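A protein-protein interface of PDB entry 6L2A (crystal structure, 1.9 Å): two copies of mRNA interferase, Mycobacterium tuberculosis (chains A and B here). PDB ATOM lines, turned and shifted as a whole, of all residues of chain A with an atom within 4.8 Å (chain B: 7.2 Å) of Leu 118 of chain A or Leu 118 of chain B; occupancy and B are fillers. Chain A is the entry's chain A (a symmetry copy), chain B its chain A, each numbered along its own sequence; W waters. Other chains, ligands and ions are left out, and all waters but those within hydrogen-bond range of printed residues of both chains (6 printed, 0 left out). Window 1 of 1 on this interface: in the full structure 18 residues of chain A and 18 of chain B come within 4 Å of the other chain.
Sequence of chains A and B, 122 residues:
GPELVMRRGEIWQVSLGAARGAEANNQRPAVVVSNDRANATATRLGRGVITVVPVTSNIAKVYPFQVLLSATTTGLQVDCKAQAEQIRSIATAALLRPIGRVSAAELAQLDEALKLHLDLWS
The guanidinium group of Arg 8 of chain B lies within hydrogen-bond range of the backbone carbonyl oxygen of Leu 118 of chain A (2.8 Å).
The side-chain amide nitrogen (ND2) of Asn 35 of chain B is in hydrogen-bond range of the backbone carbonyl oxygen (O) of Leu 116 of chain A, at 3.3 Å.
The backbone NH of Asn 35 of chain B sits at hydrogen-bond distance from the backbone carbonyl oxygen of His 117 of chain A (2.9 Å).
NE2 of His 117 of chain A sits at hydrogen-bond distance from OG1 of Thr 51 of chain B, at 2.7 Å.
The side-chain hydroxyl (OG) of Ser 89 of chain B lies within hydrogen-bond range of the backbone carbonyl oxygen (O) of Ile 87 of chain A (2.9 Å).
O of Leu 116 of chain B lies within hydrogen-bond range of ND2 of Asn 35 of chain A, at 3.3 Å.
The backbone carbonyl oxygen of His 117 of chain B sits at hydrogen-bond distance from the backbone NH of Asn 35 of chain A, 2.9 Å away.
NE2 of His 117 of chain B is in hydrogen-bond range of OG1 of Thr 51 of chain A, at 2.7 Å.
The backbone carbonyl oxygen (O) of Leu 118 of chain B lies within hydrogen-bond range of the guanidinium group (NH2) of Arg 8 of chain A (2.8 Å).
O of Val 33 of chain A lies close to O of Leu 118 of chain B, at 3.4 Å.
The backbone carbonyl oxygen (O) of Leu 118 of chain A lies close to the backbone carbonyl oxygen (O) of Val 33 of chain B, 3.4 Å away.
N of Val 33 of chain B sits at hydrogen-bond distance from O of Thr 51 of chain B, at 2.9 Å.
OG of Ser 34 of chain B sits at hydrogen-bond distance from N of Thr 51 of chain B.
The side-chain amino group (NZ) of Lys 115 of chain B lies within salt-bridge range of the side-chain carboxylate (OE2) of Glu 112 of chain B, 3.3 Å away.
The backbone NH (N) of Val 33 of chain A is in hydrogen-bond range of the backbone carbonyl oxygen (O) of Thr 51 of chain A (2.9 Å).
Ser 34 of chain A touches His 117 of chain B (CA to O, 3.6 Å).
CG2 of Thr 51 of chain A touches CG2 of Ile 87 of chain B, 3.95 Å away.
Thr 51 of chain B touches Ile 87 of chain A (CG2 to CG2, 3.95 Å).
Lys 115 of chain A touches Leu 120 of chain B.
Arg 8 of chain B touches Leu 120 of chain A.
CD2 of Leu 120 of chain A touches OD1 of Asp 111 of chain B (3.7 Å).
Leu 120 of chain B touches Leu 120 of chain A (CD1 to CD1, 3.8 Å).
Leu 118 of chain A touches just these residues of chain B: Arg 8, Val 33, Thr 51 and Leu 118.
Of the printed residues of chain B, Leu 120 of chain A touches Arg 8, Asp 111, Lys 115 and Leu 120.
Val 52 of chain B touches none of the printed residues of chain A.
Of the printed residues of chain A, Lys 115 of chain B touches Leu 120 (3.8 Å).
Leu 118 of chain B touches four residues of chain A.
Printed residues of chain A within 4 Å of Asp 119 of chain B: Arg 8 (3.6 Å) and Asn 35 (3.8 Å).
The nearest residue of chain B that does not touch Leu 118 of chain A is Ile 87 of chain B (4.1 Å).
Printed residues of chain B that touch a printed residue of chain A: Arg 8, Val 33, Ser 34, Asn 35, Thr 51, Ile 87, Ser 89, Asp 111, Lys 115, Leu 116, His 117, Leu 118, Asp 119 and Leu 120.
Printed residues of chain A that touch a printed residue of chain B: Arg 8, Val 33, Ser 34, Asn 35, Thr 51, Ile 87, Lys 115, Leu 116, His 117, Leu 118, Asp 119 and Leu 120.
Among the printed residues, no Asp or Glu carboxylate lies within 4 Å of a Lys or Arg side-chain nitrogen of the other chain.
Arg 8 of chain A touches Leu 118 of chain B, and with the chains exchanged Leu 118 of chain A touches Arg 8 of chain B.
Val 33 of chain A touches Leu 118 of chain B, and with the chains exchanged Leu 118 of chain A touches Val 33 of chain B.
Leu 120 of chain B touches its own counterpart, Leu 120 of chain A.
Positions printed for both chains: 8, 33, 34, 35, 51, 87, 114, 115, 116, 117, 118, 119 and 120.
Water W4 bridges O of Asp 119 of chain A (2.5 Å) and OD2 of Asp 111 of chain B (2.7 Å).
Water W6 bridges OD1 of Asp 119 of chain A (2.7 Å) and NH1 of Arg 8 of chain B (3.0 Å).
Water W2 bridges the side-chain carboxylate of Asp 119 of chain B (2.7 Å) and the guanidinium group of Arg 8 of chain A (3.0 Å).
Water W3 bridges OG1 of Thr 51 of chain A (2.8 Å) and NE2 of His 117 of chain B (3.3 Å).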
ATOM      1  N   ARG A   8     -13.428 -16.122  12.339  1.00  0.00           N
ATOM      2  CA  ARG A   8     -13.678 -17.262  11.469  1.00  0.00           C
ATOM      3  C   ARG A   8     -12.423 -17.617  10.680  1.00  0.00           C
ATOM      4  O   ARG A   8     -11.765 -16.740  10.112  1.00  0.00           O
ATOM      5  CB  ARG A   8     -14.827 -16.955  10.513  1.00  0.00           C
ATOM      6  CG  ARG A   8     -15.309 -18.176   9.741  1.00  0.00           C
ATOM      7  CD  ARG A   8     -16.553 -17.898   8.902  1.00  0.00           C
ATOM      8  NE  ARG A   8     -17.181 -19.143   8.460  1.00  0.00           N
ATOM      9  CZ  ARG A   8     -16.868 -19.790   7.340  1.00  0.00           C
ATOM     10  NH1 ARG A   8     -15.936 -19.310   6.527  1.00  0.00           N
ATOM     11  NH2 ARG A   8     -17.487 -20.921   7.032  1.00  0.00           N
ATOM     12  N   VAL A  33     -15.817 -21.548  12.629  1.00  0.00           N
ATOM     13  CA  VAL A  33     -16.576 -21.466  11.382  1.00  0.00           C
ATOM     14  C   VAL A  33     -17.882 -20.697  11.554  1.00  0.00           C
ATOM     15  O   VAL A  33     -18.593 -20.446  10.574  1.00  0.00           O
ATOM     16  CB  VAL A  33     -16.848 -22.866  10.798  1.00  0.00           C
ATOM     17  CG1 VAL A  33     -15.541 -23.542  10.418  1.00  0.00           C
ATOM     18  CG2 VAL A  33     -17.641 -23.719  11.779  1.00  0.00           C
ATOM     19  N   SER A  34     -18.221 -20.319  12.783  1.00  0.00           N
ATOM     20  CA  SER A  34     -19.335 -19.399  12.957  1.00  0.00           C
ATOM     21  C   SER A  34     -18.973 -18.041  12.360  1.00  0.00           C
ATOM     22  O   SER A  34     -17.808 -17.638  12.348  1.00  0.00           O
ATOM     23  CB  SER A  34     -19.705 -19.262  14.437  1.00  0.00           C
ATOM     24  OG  SER A  34     -18.560 -19.123  15.261  1.00  0.00           O
ATOM     25  N   ASN A  35     -19.982 -17.345  11.837  1.00  0.00           N
ATOM     26  CA  ASN A  35     -19.734 -16.069  11.181  1.00  0.00           C
ATOM     27  C   ASN A  35     -19.231 -15.033  12.186  1.00  0.00           C
ATOM     28  O   ASN A  35     -19.444 -15.142  13.397  1.00  0.00           O
ATOM     29  CB  ASN A  35     -20.996 -15.566  10.472  1.00  0.00           C
ATOM     30  CG  ASN A  35     -22.052 -15.059  11.437  1.00  0.00           C
ATOM     31  OD1 ASN A  35     -21.993 -13.921  11.897  1.00  0.00           O
ATOM     32  ND2 ASN A  35     -23.032 -15.902  11.739  1.00  0.00           N
ATOM     33  N   THR A  51     -19.075 -21.772  16.939  1.00  0.00           N
ATOM     34  CA  THR A  51     -19.145 -23.036  16.223  1.00  0.00           C
ATOM     35  C   THR A  51     -17.774 -23.344  15.637  1.00  0.00           C
ATOM     36  O   THR A  51     -17.166 -22.485  14.992  1.00  0.00           O
ATOM     37  CB  THR A  51     -20.213 -22.992  15.130  1.00  0.00           C
ATOM     38  OG1 THR A  51     -21.489 -22.743  15.732  1.00  0.00           O
ATOM     39  CG2 THR A  51     -20.263 -24.312  14.396  1.00  0.00           C
ATOM     40  N   ILE A  87     -18.548 -31.110  13.416  1.00  0.00           N
ATOM     41  CA  ILE A  87     -18.812 -29.728  13.801  1.00  0.00           C
ATOM     42  C   ILE A  87     -19.547 -29.674  15.137  1.00  0.00           C
ATOM     43  O   ILE A  87     -20.449 -30.477  15.407  1.00  0.00           O
ATOM     44  CB  ILE A  87     -19.605 -29.038  12.677  1.00  0.00           C
ATOM     45  CG1 ILE A  87     -19.963 -27.596  13.034  1.00  0.00           C
ATOM     46  CG2 ILE A  87     -20.861 -29.835  12.334  1.00  0.00           C
ATOM     47  CD1 ILE A  87     -20.657 -26.865  11.900  1.00  0.00           C
ATOM     48  N   LEU A 114     -18.380 -27.938   4.415  1.00  0.00           N
ATOM     49  CA  LEU A 114     -19.527 -27.716   5.289  1.00  0.00           C
ATOM     50  C   LEU A 114     -20.835 -27.801   4.513  1.00  0.00           C
ATOM     51  O   LEU A 114     -21.804 -28.407   4.986  1.00  0.00           O
ATOM     52  CB  LEU A 114     -19.398 -26.361   5.983  1.00  0.00           C
ATOM     53  CG  LEU A 114     -18.346 -26.277   7.091  1.00  0.00           C
ATOM     54  CD1 LEU A 114     -18.063 -24.825   7.446  1.00  0.00           C
ATOM     55  CD2 LEU A 114     -18.805 -27.051   8.314  1.00  0.00           C
ATOM     56  N   LYS A 115     -20.886 -27.194   3.323  1.00  0.00           N
ATOM     57  CA  LYS A 115     -22.098 -27.266   2.513  1.00  0.00           C
ATOM     58  C   LYS A 115     -22.399 -28.700   2.101  1.00  0.00           C
ATOM     59  O   LYS A 115     -23.561 -29.127   2.113  1.00  0.00           O
ATOM     60  CB  LYS A 115     -21.965 -26.368   1.284  1.00  0.00           C
ATOM     61  CG  LYS A 115     -21.883 -24.888   1.613  1.00  0.00           C
ATOM     62  CD  LYS A 115     -22.162 -24.041   0.390  1.00  0.00           C
ATOM     63  CE  LYS A 115     -21.277 -24.462  -0.765  1.00  0.00           C
ATOM     64  NZ  LYS A 115     -21.801 -23.967  -2.068  1.00  0.00           N
ATOM     65  N   LEU A 116     -21.366 -29.463   1.740  1.00  0.00           N
ATOM     66  CA  LEU A 116     -21.562 -30.867   1.400  1.00  0.00           C
ATOM     67  C   LEU A 116     -22.090 -31.652   2.595  1.00  0.00           C
ATOM     68  O   LEU A 116     -23.068 -32.400   2.479  1.00  0.00           O
ATOM     69  CB  LEU A 116     -20.251 -31.474   0.901  1.00  0.00           C
ATOM     70  CG  LEU A 116     -20.295 -32.986   0.661  1.00  0.00           C
ATOM     71  CD1 LEU A 116     -21.078 -33.316  -0.603  1.00  0.00           C
ATOM     72  CD2 LEU A 116     -18.890 -33.564   0.601  1.00  0.00           C
ATOM     73  N   HIS A 117     -21.453 -31.493   3.756  1.00  0.00           N
ATOM     74  CA  HIS A 117     -21.860 -32.270   4.922  1.00  0.00           C
ATOM     75  C   HIS A 117     -23.283 -31.936   5.346  1.00  0.00           C
ATOM     76  O   HIS A 117     -24.024 -32.814   5.800  1.00  0.00           O
ATOM     77  CB  HIS A 117     -20.905 -32.035   6.088  1.00  0.00           C
ATOM     78  CG  HIS A 117     -21.350 -32.689   7.359  1.00  0.00           C
ATOM     79  ND1 HIS A 117     -21.446 -34.058   7.497  1.00  0.00           N
ATOM     80  CD2 HIS A 117     -21.752 -32.164   8.541  1.00  0.00           C
ATOM     81  CE1 HIS A 117     -21.871 -34.347   8.714  1.00  0.00           C
ATOM     82  NE2 HIS A 117     -22.067 -33.215   9.367  1.00  0.00           N
ATOM     83  N   LEU A 118     -23.685 -30.674   5.210  1.00  0.00           N
ATOM     84  CA  LEU A 118     -24.987 -30.230   5.686  1.00  0.00           C
ATOM     85  C   LEU A 118     -26.045 -30.217   4.590  1.00  0.00           C
ATOM     86  O   LEU A 118     -27.159 -29.734   4.825  1.00  0.00           O
ATOM     87  CB  LEU A 118     -24.861 -28.850   6.327  1.00  0.00           C
ATOM     88  CG  LEU A 118     -24.004 -28.854   7.595  1.00  0.00           C
ATOM     89  CD1 LEU A 118     -23.741 -27.442   8.057  1.00  0.00           C
ATOM     90  CD2 LEU A 118     -24.668 -29.658   8.701  1.00  0.00           C
ATOM     91  N   ASP A 119     -25.722 -30.743   3.406  1.00  0.00           N
ATOM     92  CA  ASP A 119     -26.668 -30.856   2.294  1.00  0.00           C
ATOM     93  C   ASP A 119     -27.169 -29.482   1.850  1.00  0.00           C
ATOM     94  O   ASP A 119     -28.337 -29.309   1.498  1.00  0.00           O
ATOM     95  CB  ASP A 119     -27.838 -31.777   2.656  1.00  0.00           C
ATOM     96  CG  ASP A 119     -28.477 -32.420   1.440  1.00  0.00           C
ATOM     97  OD1 ASP A 119     -29.688 -32.725   1.492  1.00  0.00           O
ATOM     98  OD2 ASP A 119     -27.769 -32.623   0.433  1.00  0.00           O
ATOM     99  N   LEU A 120     -26.271 -28.499   1.853  1.00  0.00           N
ATOM    100  CA  LEU A 120     -26.598 -27.125   1.491  1.00  0.00           C
ATOM    101  C   LEU A 120     -26.151 -26.882   0.054  1.00  0.00           C
ATOM    102  O   LEU A 120     -24.952 -26.925  -0.246  1.00  0.00           O
ATOM    103  CB  LEU A 120     -25.932 -26.141   2.450  1.00  0.00           C
ATOM    104  CG  LEU A 120     -26.272 -26.342   3.928  1.00  0.00           C
ATOM    105  CD1 LEU A 120     -25.454 -25.410   4.809  1.00  0.00           C
ATOM    106  CD2 LEU A 120     -27.761 -26.137   4.164  1.00  0.00           C
ATOM    107  N   ARG B   8     -32.576 -36.602   7.357  1.00  0.00           N
ATOM    108  CA  ARG B   8     -32.455 -35.154   7.461  1.00  0.00           C
ATOM    109  C   ARG B   8     -33.832 -34.506   7.515  1.00  0.00           C
ATOM    110  O   ARG B   8     -34.719 -34.838   6.722  1.00  0.00           O
ATOM    111  CB  ARG B   8     -31.665 -34.604   6.275  1.00  0.00           C
ATOM    112  CG  ARG B   8     -31.286 -33.138   6.435  1.00  0.00           C
ATOM    113  CD  ARG B   8     -30.369 -32.636   5.324  1.00  0.00           C
ATOM    114  NE  ARG B   8     -29.756 -31.358   5.683  1.00  0.00           N
ATOM    115  CZ  ARG B   8     -30.297 -30.166   5.442  1.00  0.00           C
ATOM    116  NH1 ARG B   8     -31.468 -30.074   4.827  1.00  0.00           N
ATOM    117  NH2 ARG B   8     -29.667 -29.062   5.818  1.00  0.00           N
ATOM    118  N   VAL B  33     -29.604 -32.563  10.535  1.00  0.00           N
ATOM    119  CA  VAL B  33     -29.243 -31.698   9.414  1.00  0.00           C
ATOM    120  C   VAL B  33     -28.037 -32.227   8.644  1.00  0.00           C
ATOM    121  O   VAL B  33     -27.665 -31.670   7.605  1.00  0.00           O
ATOM    122  CB  VAL B  33     -28.990 -30.251   9.881  1.00  0.00           C
ATOM    123  CG1 VAL B  33     -30.266 -29.649  10.447  1.00  0.00           C
ATOM    124  CG2 VAL B  33     -27.862 -30.199  10.902  1.00  0.00           C
ATOM    125  N   SER B  34     -27.410 -33.292   9.133  1.00  0.00           N
ATOM    126  CA  SER B  34     -26.404 -33.956   8.318  1.00  0.00           C
ATOM    127  C   SER B  34     -27.070 -34.586   7.097  1.00  0.00           C
ATOM    128  O   SER B  34     -28.229 -35.004   7.146  1.00  0.00           O
ATOM    129  CB  SER B  34     -25.648 -35.011   9.131  1.00  0.00           C
ATOM    130  OG  SER B  34     -26.522 -35.797   9.923  1.00  0.00           O
ATOM    131  N   ASN B  35     -26.336 -34.629   5.986  1.00  0.00           N
ATOM    132  CA  ASN B  35     -26.902 -35.146   4.748  1.00  0.00           C
ATOM    133  C   ASN B  35     -27.214 -36.637   4.879  1.00  0.00           C
ATOM    134  O   ASN B  35     -26.656 -37.348   5.719  1.00  0.00           O
ATOM    135  CB  ASN B  35     -25.957 -34.893   3.569  1.00  0.00           C
ATOM    136  CG  ASN B  35     -24.735 -35.794   3.588  1.00  0.00           C
ATOM    137  OD1 ASN B  35     -24.792 -36.943   3.152  1.00  0.00           O
ATOM    138  ND2 ASN B  35     -23.621 -35.272   4.085  1.00  0.00           N
ATOM    139  N   THR B  51     -25.257 -34.935  12.709  1.00  0.00           N
ATOM    140  CA  THR B  51     -25.251 -33.521  13.051  1.00  0.00           C
ATOM    141  C   THR B  51     -26.686 -33.056  13.246  1.00  0.00           C
ATOM    142  O   THR B  51     -27.545 -33.319  12.398  1.00  0.00           O
ATOM    143  CB  THR B  51     -24.547 -32.697  11.973  1.00  0.00           C
ATOM    144  OG1 THR B  51     -23.189 -33.139  11.857  1.00  0.00           O
ATOM    145  CG2 THR B  51     -24.557 -31.231  12.347  1.00  0.00           C
ATOM    146  N   VAL B  52     -26.947 -32.391  14.373  1.00  0.00           N
ATOM    147  CA  VAL B  52     -28.298 -32.007  14.754  1.00  0.00           C
ATOM    148  C   VAL B  52     -28.335 -30.532  15.127  1.00  0.00           C
ATOM    149  O   VAL B  52     -27.325 -29.927  15.496  1.00  0.00           O
ATOM    150  CB  VAL B  52     -28.841 -32.858  15.923  1.00  0.00           C
ATOM    151  CG1 VAL B  52     -28.877 -34.332  15.540  1.00  0.00           C
ATOM    152  CG2 VAL B  52     -28.004 -32.636  17.177  1.00  0.00           C
ATOM    153  N   VAL B  53     -29.533 -29.964  15.033  1.00  0.00           N
ATOM    154  CA  VAL B  53     -29.806 -28.590  15.448  1.00  0.00           C
ATOM    155  C   VAL B  53     -30.807 -28.627  16.598  1.00  0.00           C
ATOM    156  O   VAL B  53     -31.956 -29.046  16.402  1.00  0.00           O
ATOM    157  CB  VAL B  53     -30.326 -27.755  14.267  1.00  0.00           C
ATOM    158  CG1 VAL B  53     -30.918 -26.454  14.756  1.00  0.00           C
ATOM    159  CG2 VAL B  53     -29.198 -27.489  13.281  1.00  0.00           C
ATOM    160  N   PHE B  65     -30.835 -16.717  12.370  1.00  0.00           N
ATOM    161  CA  PHE B  65     -30.153 -18.000  12.428  1.00  0.00           C
ATOM    162  C   PHE B  65     -30.975 -19.052  13.162  1.00  0.00           C
ATOM    163  O   PHE B  65     -30.431 -20.085  13.571  1.00  0.00           O
ATOM    164  CB  PHE B  65     -28.775 -17.842  13.078  1.00  0.00           C
ATOM    165  CG  PHE B  65     -28.779 -17.002  14.324  1.00  0.00           C
ATOM    166  CD1 PHE B  65     -29.028 -17.574  15.562  1.00  0.00           C
ATOM    167  CD2 PHE B  65     -28.524 -15.642  14.261  1.00  0.00           C
ATOM    168  CE1 PHE B  65     -29.028 -16.805  16.709  1.00  0.00           C
ATOM    169  CE2 PHE B  65     -28.523 -14.866  15.407  1.00  0.00           C
ATOM    170  CZ  PHE B  65     -28.773 -15.449  16.632  1.00  0.00           C
ATOM    171  N   ALA B  84     -29.925 -22.918  14.938  1.00  0.00           N
ATOM    172  CA  ALA B  84     -28.781 -23.307  14.123  1.00  0.00           C
ATOM    173  C   ALA B  84     -27.456 -22.890  14.746  1.00  0.00           C
ATOM    174  O   ALA B  84     -26.428 -23.514  14.458  1.00  0.00           O
ATOM    175  CB  ALA B  84     -28.899 -22.719  12.716  1.00  0.00           C
ATOM    176  N   ILE B  87     -25.699 -25.800  16.742  1.00  0.00           N
ATOM    177  CA  ILE B  87     -25.495 -27.040  15.999  1.00  0.00           C
ATOM    178  C   ILE B  87     -24.423 -27.895  16.667  1.00  0.00           C
ATOM    179  O   ILE B  87     -23.397 -27.389  17.138  1.00  0.00           O
ATOM    180  CB  ILE B  87     -25.135 -26.696  14.543  1.00  0.00           C
ATOM    181  CG1 ILE B  87     -24.857 -27.950  13.715  1.00  0.00           C
ATOM    182  CG2 ILE B  87     -23.945 -25.742  14.490  1.00  0.00           C
ATOM    183  CD1 ILE B  87     -24.599 -27.642  12.251  1.00  0.00           C
ATOM    184  N   SER B  89     -22.597 -32.144  16.635  1.00  0.00           N
ATOM    185  CA  SER B  89     -22.471 -33.500  16.124  1.00  0.00           C
ATOM    186  C   SER B  89     -22.490 -34.469  17.296  1.00  0.00           C
ATOM    187  O   SER B  89     -21.794 -34.257  18.295  1.00  0.00           O
ATOM    188  CB  SER B  89     -21.190 -33.673  15.306  1.00  0.00           C
ATOM    189  OG  SER B  89     -21.252 -32.909  14.114  1.00  0.00           O
ATOM    190  N   ASP B 111     -32.081 -24.518   6.085  1.00  0.00           N
ATOM    191  CA  ASP B 111     -30.911 -24.421   5.216  1.00  0.00           C
ATOM    192  C   ASP B 111     -30.381 -22.995   5.171  1.00  0.00           C
ATOM    193  O   ASP B 111     -29.166 -22.774   5.252  1.00  0.00           O
ATOM    194  CB  ASP B 111     -31.247 -24.898   3.803  1.00  0.00           C
ATOM    195  CG  ASP B 111     -31.567 -26.379   3.738  1.00  0.00           C
ATOM    196  OD1 ASP B 111     -31.281 -27.105   4.713  1.00  0.00           O
ATOM    197  OD2 ASP B 111     -32.094 -26.819   2.694  1.00  0.00           O
ATOM    198  N   GLU B 112     -31.277 -22.012   5.046  1.00  0.00           N
ATOM    199  CA  GLU B 112     -30.843 -20.619   4.992  1.00  0.00           C
ATOM    200  C   GLU B 112     -30.271 -20.164   6.328  1.00  0.00           C
ATOM    201  O   GLU B 112     -29.285 -19.418   6.363  1.00  0.00           O
ATOM    202  CB  GLU B 112     -32.008 -19.726   4.570  1.00  0.00           C
ATOM    203  CG  GLU B 112     -32.411 -19.896   3.118  1.00  0.00           C
ATOM    204  CD  GLU B 112     -31.304 -19.496   2.164  1.00  0.00           C
ATOM    205  OE1 GLU B 112     -30.788 -18.366   2.292  1.00  0.00           O
ATOM    206  OE2 GLU B 112     -30.947 -20.313   1.290  1.00  0.00           O
ATOM    207  N   ALA B 113     -30.875 -20.600   7.436  1.00  0.00           N
ATOM    208  CA  ALA B 113     -30.355 -20.240   8.752  1.00  0.00           C
ATOM    209  C   ALA B 113     -28.975 -20.846   8.981  1.00  0.00           C
ATOM    210  O   ALA B 113     -28.101 -20.211   9.583  1.00  0.00           O
ATOM    211  CB  ALA B 113     -31.326 -20.689   9.843  1.00  0.00           C
ATOM    212  N   LEU B 114     -28.761 -22.074   8.507  1.00  0.00           N
ATOM    213  CA  LEU B 114     -27.447 -22.694   8.629  1.00  0.00           C
ATOM    214  C   LEU B 114     -26.411 -21.962   7.787  1.00  0.00           C
ATOM    215  O   LEU B 114     -25.285 -21.728   8.244  1.00  0.00           O
ATOM    216  CB  LEU B 114     -27.527 -24.167   8.226  1.00  0.00           C
ATOM    217  CG  LEU B 114     -28.225 -25.093   9.223  1.00  0.00           C
ATOM    218  CD1 LEU B 114     -28.559 -26.424   8.568  1.00  0.00           C
ATOM    219  CD2 LEU B 114     -27.354 -25.299  10.452  1.00  0.00           C
ATOM    220  N   LYS B 115     -26.767 -21.597   6.552  1.00  0.00           N
ATOM    221  CA  LYS B 115     -25.833 -20.862   5.704  1.00  0.00           C
ATOM    222  C   LYS B 115     -25.500 -19.503   6.303  1.00  0.00           C
ATOM    223  O   LYS B 115     -24.342 -19.068   6.270  1.00  0.00           O
ATOM    224  CB  LYS B 115     -26.408 -20.705   4.297  1.00  0.00           C
ATOM    225  CG  LYS B 115     -26.561 -22.017   3.548  1.00  0.00           C
ATOM    226  CD  LYS B 115     -26.737 -21.781   2.063  1.00  0.00           C
ATOM    227  CE  LYS B 115     -27.859 -20.795   1.808  1.00  0.00           C
ATOM    228  NZ  LYS B 115     -27.784 -20.219   0.437  1.00  0.00           N
ATOM    229  N   LEU B 116     -26.501 -18.820   6.862  1.00  0.00           N
ATOM    230  CA  LEU B 116     -26.251 -17.543   7.521  1.00  0.00           C
ATOM    231  C   LEU B 116     -25.321 -17.715   8.716  1.00  0.00           C
ATOM    232  O   LEU B 116     -24.338 -16.980   8.865  1.00  0.00           O
ATOM    233  CB  LEU B 116     -27.573 -16.912   7.960  1.00  0.00           C
ATOM    234  CG  LEU B 116     -27.428 -15.641   8.802  1.00  0.00           C
ATOM    235  CD1 LEU B 116     -27.001 -14.460   7.940  1.00  0.00           C
ATOM    236  CD2 LEU B 116     -28.717 -15.337   9.547  1.00  0.00           C
ATOM    237  N   HIS B 117     -25.618 -18.685   9.582  1.00  0.00           N
ATOM    238  CA  HIS B 117     -24.813 -18.857  10.787  1.00  0.00           C
ATOM    239  C   HIS B 117     -23.376 -19.226  10.449  1.00  0.00           C
ATOM    240  O   HIS B 117     -22.441 -18.807  11.142  1.00  0.00           O
ATOM    241  CB  HIS B 117     -25.420 -19.922  11.695  1.00  0.00           C
ATOM    242  CG  HIS B 117     -24.563 -20.250  12.878  1.00  0.00           C
ATOM    243  ND1 HIS B 117     -24.277 -19.332  13.866  1.00  0.00           N
ATOM    244  CD2 HIS B 117     -23.905 -21.385  13.217  1.00  0.00           C
ATOM    245  CE1 HIS B 117     -23.497 -19.893  14.772  1.00  0.00           C
ATOM    246  NE2 HIS B 117     -23.253 -21.137  14.400  1.00  0.00           N
ATOM    247  N   LEU B 118     -23.174 -20.011   9.393  1.00  0.00           N
ATOM    248  CA  LEU B 118     -21.849 -20.508   9.051  1.00  0.00           C
ATOM    249  C   LEU B 118     -21.153 -19.660   7.994  1.00  0.00           C
ATOM    250  O   LEU B 118     -20.080 -20.045   7.515  1.00  0.00           O
ATOM    251  CB  LEU B 118     -21.944 -21.962   8.595  1.00  0.00           C
ATOM    252  CG  LEU B 118     -22.401 -22.910   9.705  1.00  0.00           C
ATOM    253  CD1 LEU B 118     -22.682 -24.282   9.143  1.00  0.00           C
ATOM    254  CD2 LEU B 118     -21.366 -22.993  10.814  1.00  0.00           C
ATOM    255  N   ASP B 119     -21.736 -18.514   7.631  1.00  0.00           N
ATOM    256  CA  ASP B 119     -21.136 -17.575   6.680  1.00  0.00           C
ATOM    257  C   ASP B 119     -20.940 -18.224   5.310  1.00  0.00           C
ATOM    258  O   ASP B 119     -19.946 -17.980   4.623  1.00  0.00           O
ATOM    259  CB  ASP B 119     -19.815 -17.015   7.218  1.00  0.00           C
ATOM    260  CG  ASP B 119     -19.477 -15.654   6.641  1.00  0.00           C
ATOM    261  OD1 ASP B 119     -18.275 -15.329   6.539  1.00  0.00           O
ATOM    262  OD2 ASP B 119     -20.413 -14.907   6.289  1.00  0.00           O
ATOM    263  N   LEU B 120     -21.905 -19.045   4.905  1.00  0.00           N
ATOM    264  CA  LEU B 120     -21.851 -19.767   3.638  1.00  0.00           C
ATOM    265  C   LEU B 120     -22.711 -19.027   2.620  1.00  0.00           C
ATOM    266  O   LEU B 120     -23.932 -18.929   2.783  1.00  0.00           O
ATOM    267  CB  LEU B 120     -22.326 -21.208   3.819  1.00  0.00           C
ATOM    268  CG  LEU B 120     -21.562 -22.018   4.867  1.00  0.00           C
ATOM    269  CD1 LEU B 120     -22.197 -23.385   5.072  1.00  0.00           C
ATOM    270  CD2 LEU B 120     -20.101 -22.159   4.471  1.00  0.00           C
ATOM    271  N   TRP B 121     -22.074 -18.498   1.582  1.00  0.00           N
ATOM    272  CA  TRP B 121     -22.791 -17.802   0.517  1.00  0.00           C
ATOM    273  C   TRP B 121     -22.528 -18.471  -0.830  1.00  0.00           C
ATOM    274  O   TRP B 121     -23.445 -18.989  -1.470  1.00  0.00           O
ATOM    275  CB  TRP B 121     -22.386 -16.327   0.459  1.00  0.00           C
ATOM    276  CG  TRP B 121     -22.384 -15.641   1.792  1.00  0.00           C
ATOM    277  CD1 TRP B 121     -21.352 -15.581   2.681  1.00  0.00           C
ATOM    278  CD2 TRP B 121     -23.468 -14.917   2.388  1.00  0.00           C
ATOM    279  NE1 TRP B 121     -21.724 -14.864   3.793  1.00  0.00           N
ATOM    280  CE2 TRP B 121     -23.019 -14.445   3.638  1.00  0.00           C
ATOM    281  CE3 TRP B 121     -24.774 -14.621   1.986  1.00  0.00           C
ATOM    282  CZ2 TRP B 121     -23.827 -13.696   4.488  1.00  0.00           C
ATOM    283  CZ3 TRP B 121     -25.576 -13.876   2.835  1.00  0.00           C
ATOM    284  CH2 TRP B 121     -25.100 -13.423   4.070  1.00  0.00           C
HETATM  285  O   HOH W   1     -21.663 -21.485  -1.745  1.00  0.00           O
HETATM  286  O   HOH W   2     -15.853 -16.428   5.870  1.00  0.00           O
HETATM  287  O   HOH W   3     -22.507 -20.918  17.652  1.00  0.00           O
HETATM  288  O   HOH W   4     -30.500 -28.114   0.871  1.00  0.00           O
HETATM  289  O   HOH W   5     -21.883 -35.650  11.650  1.00  0.00           O
HETATM  290  O   HOH W   6     -32.059 -31.746   2.460  1.00  0.00           O
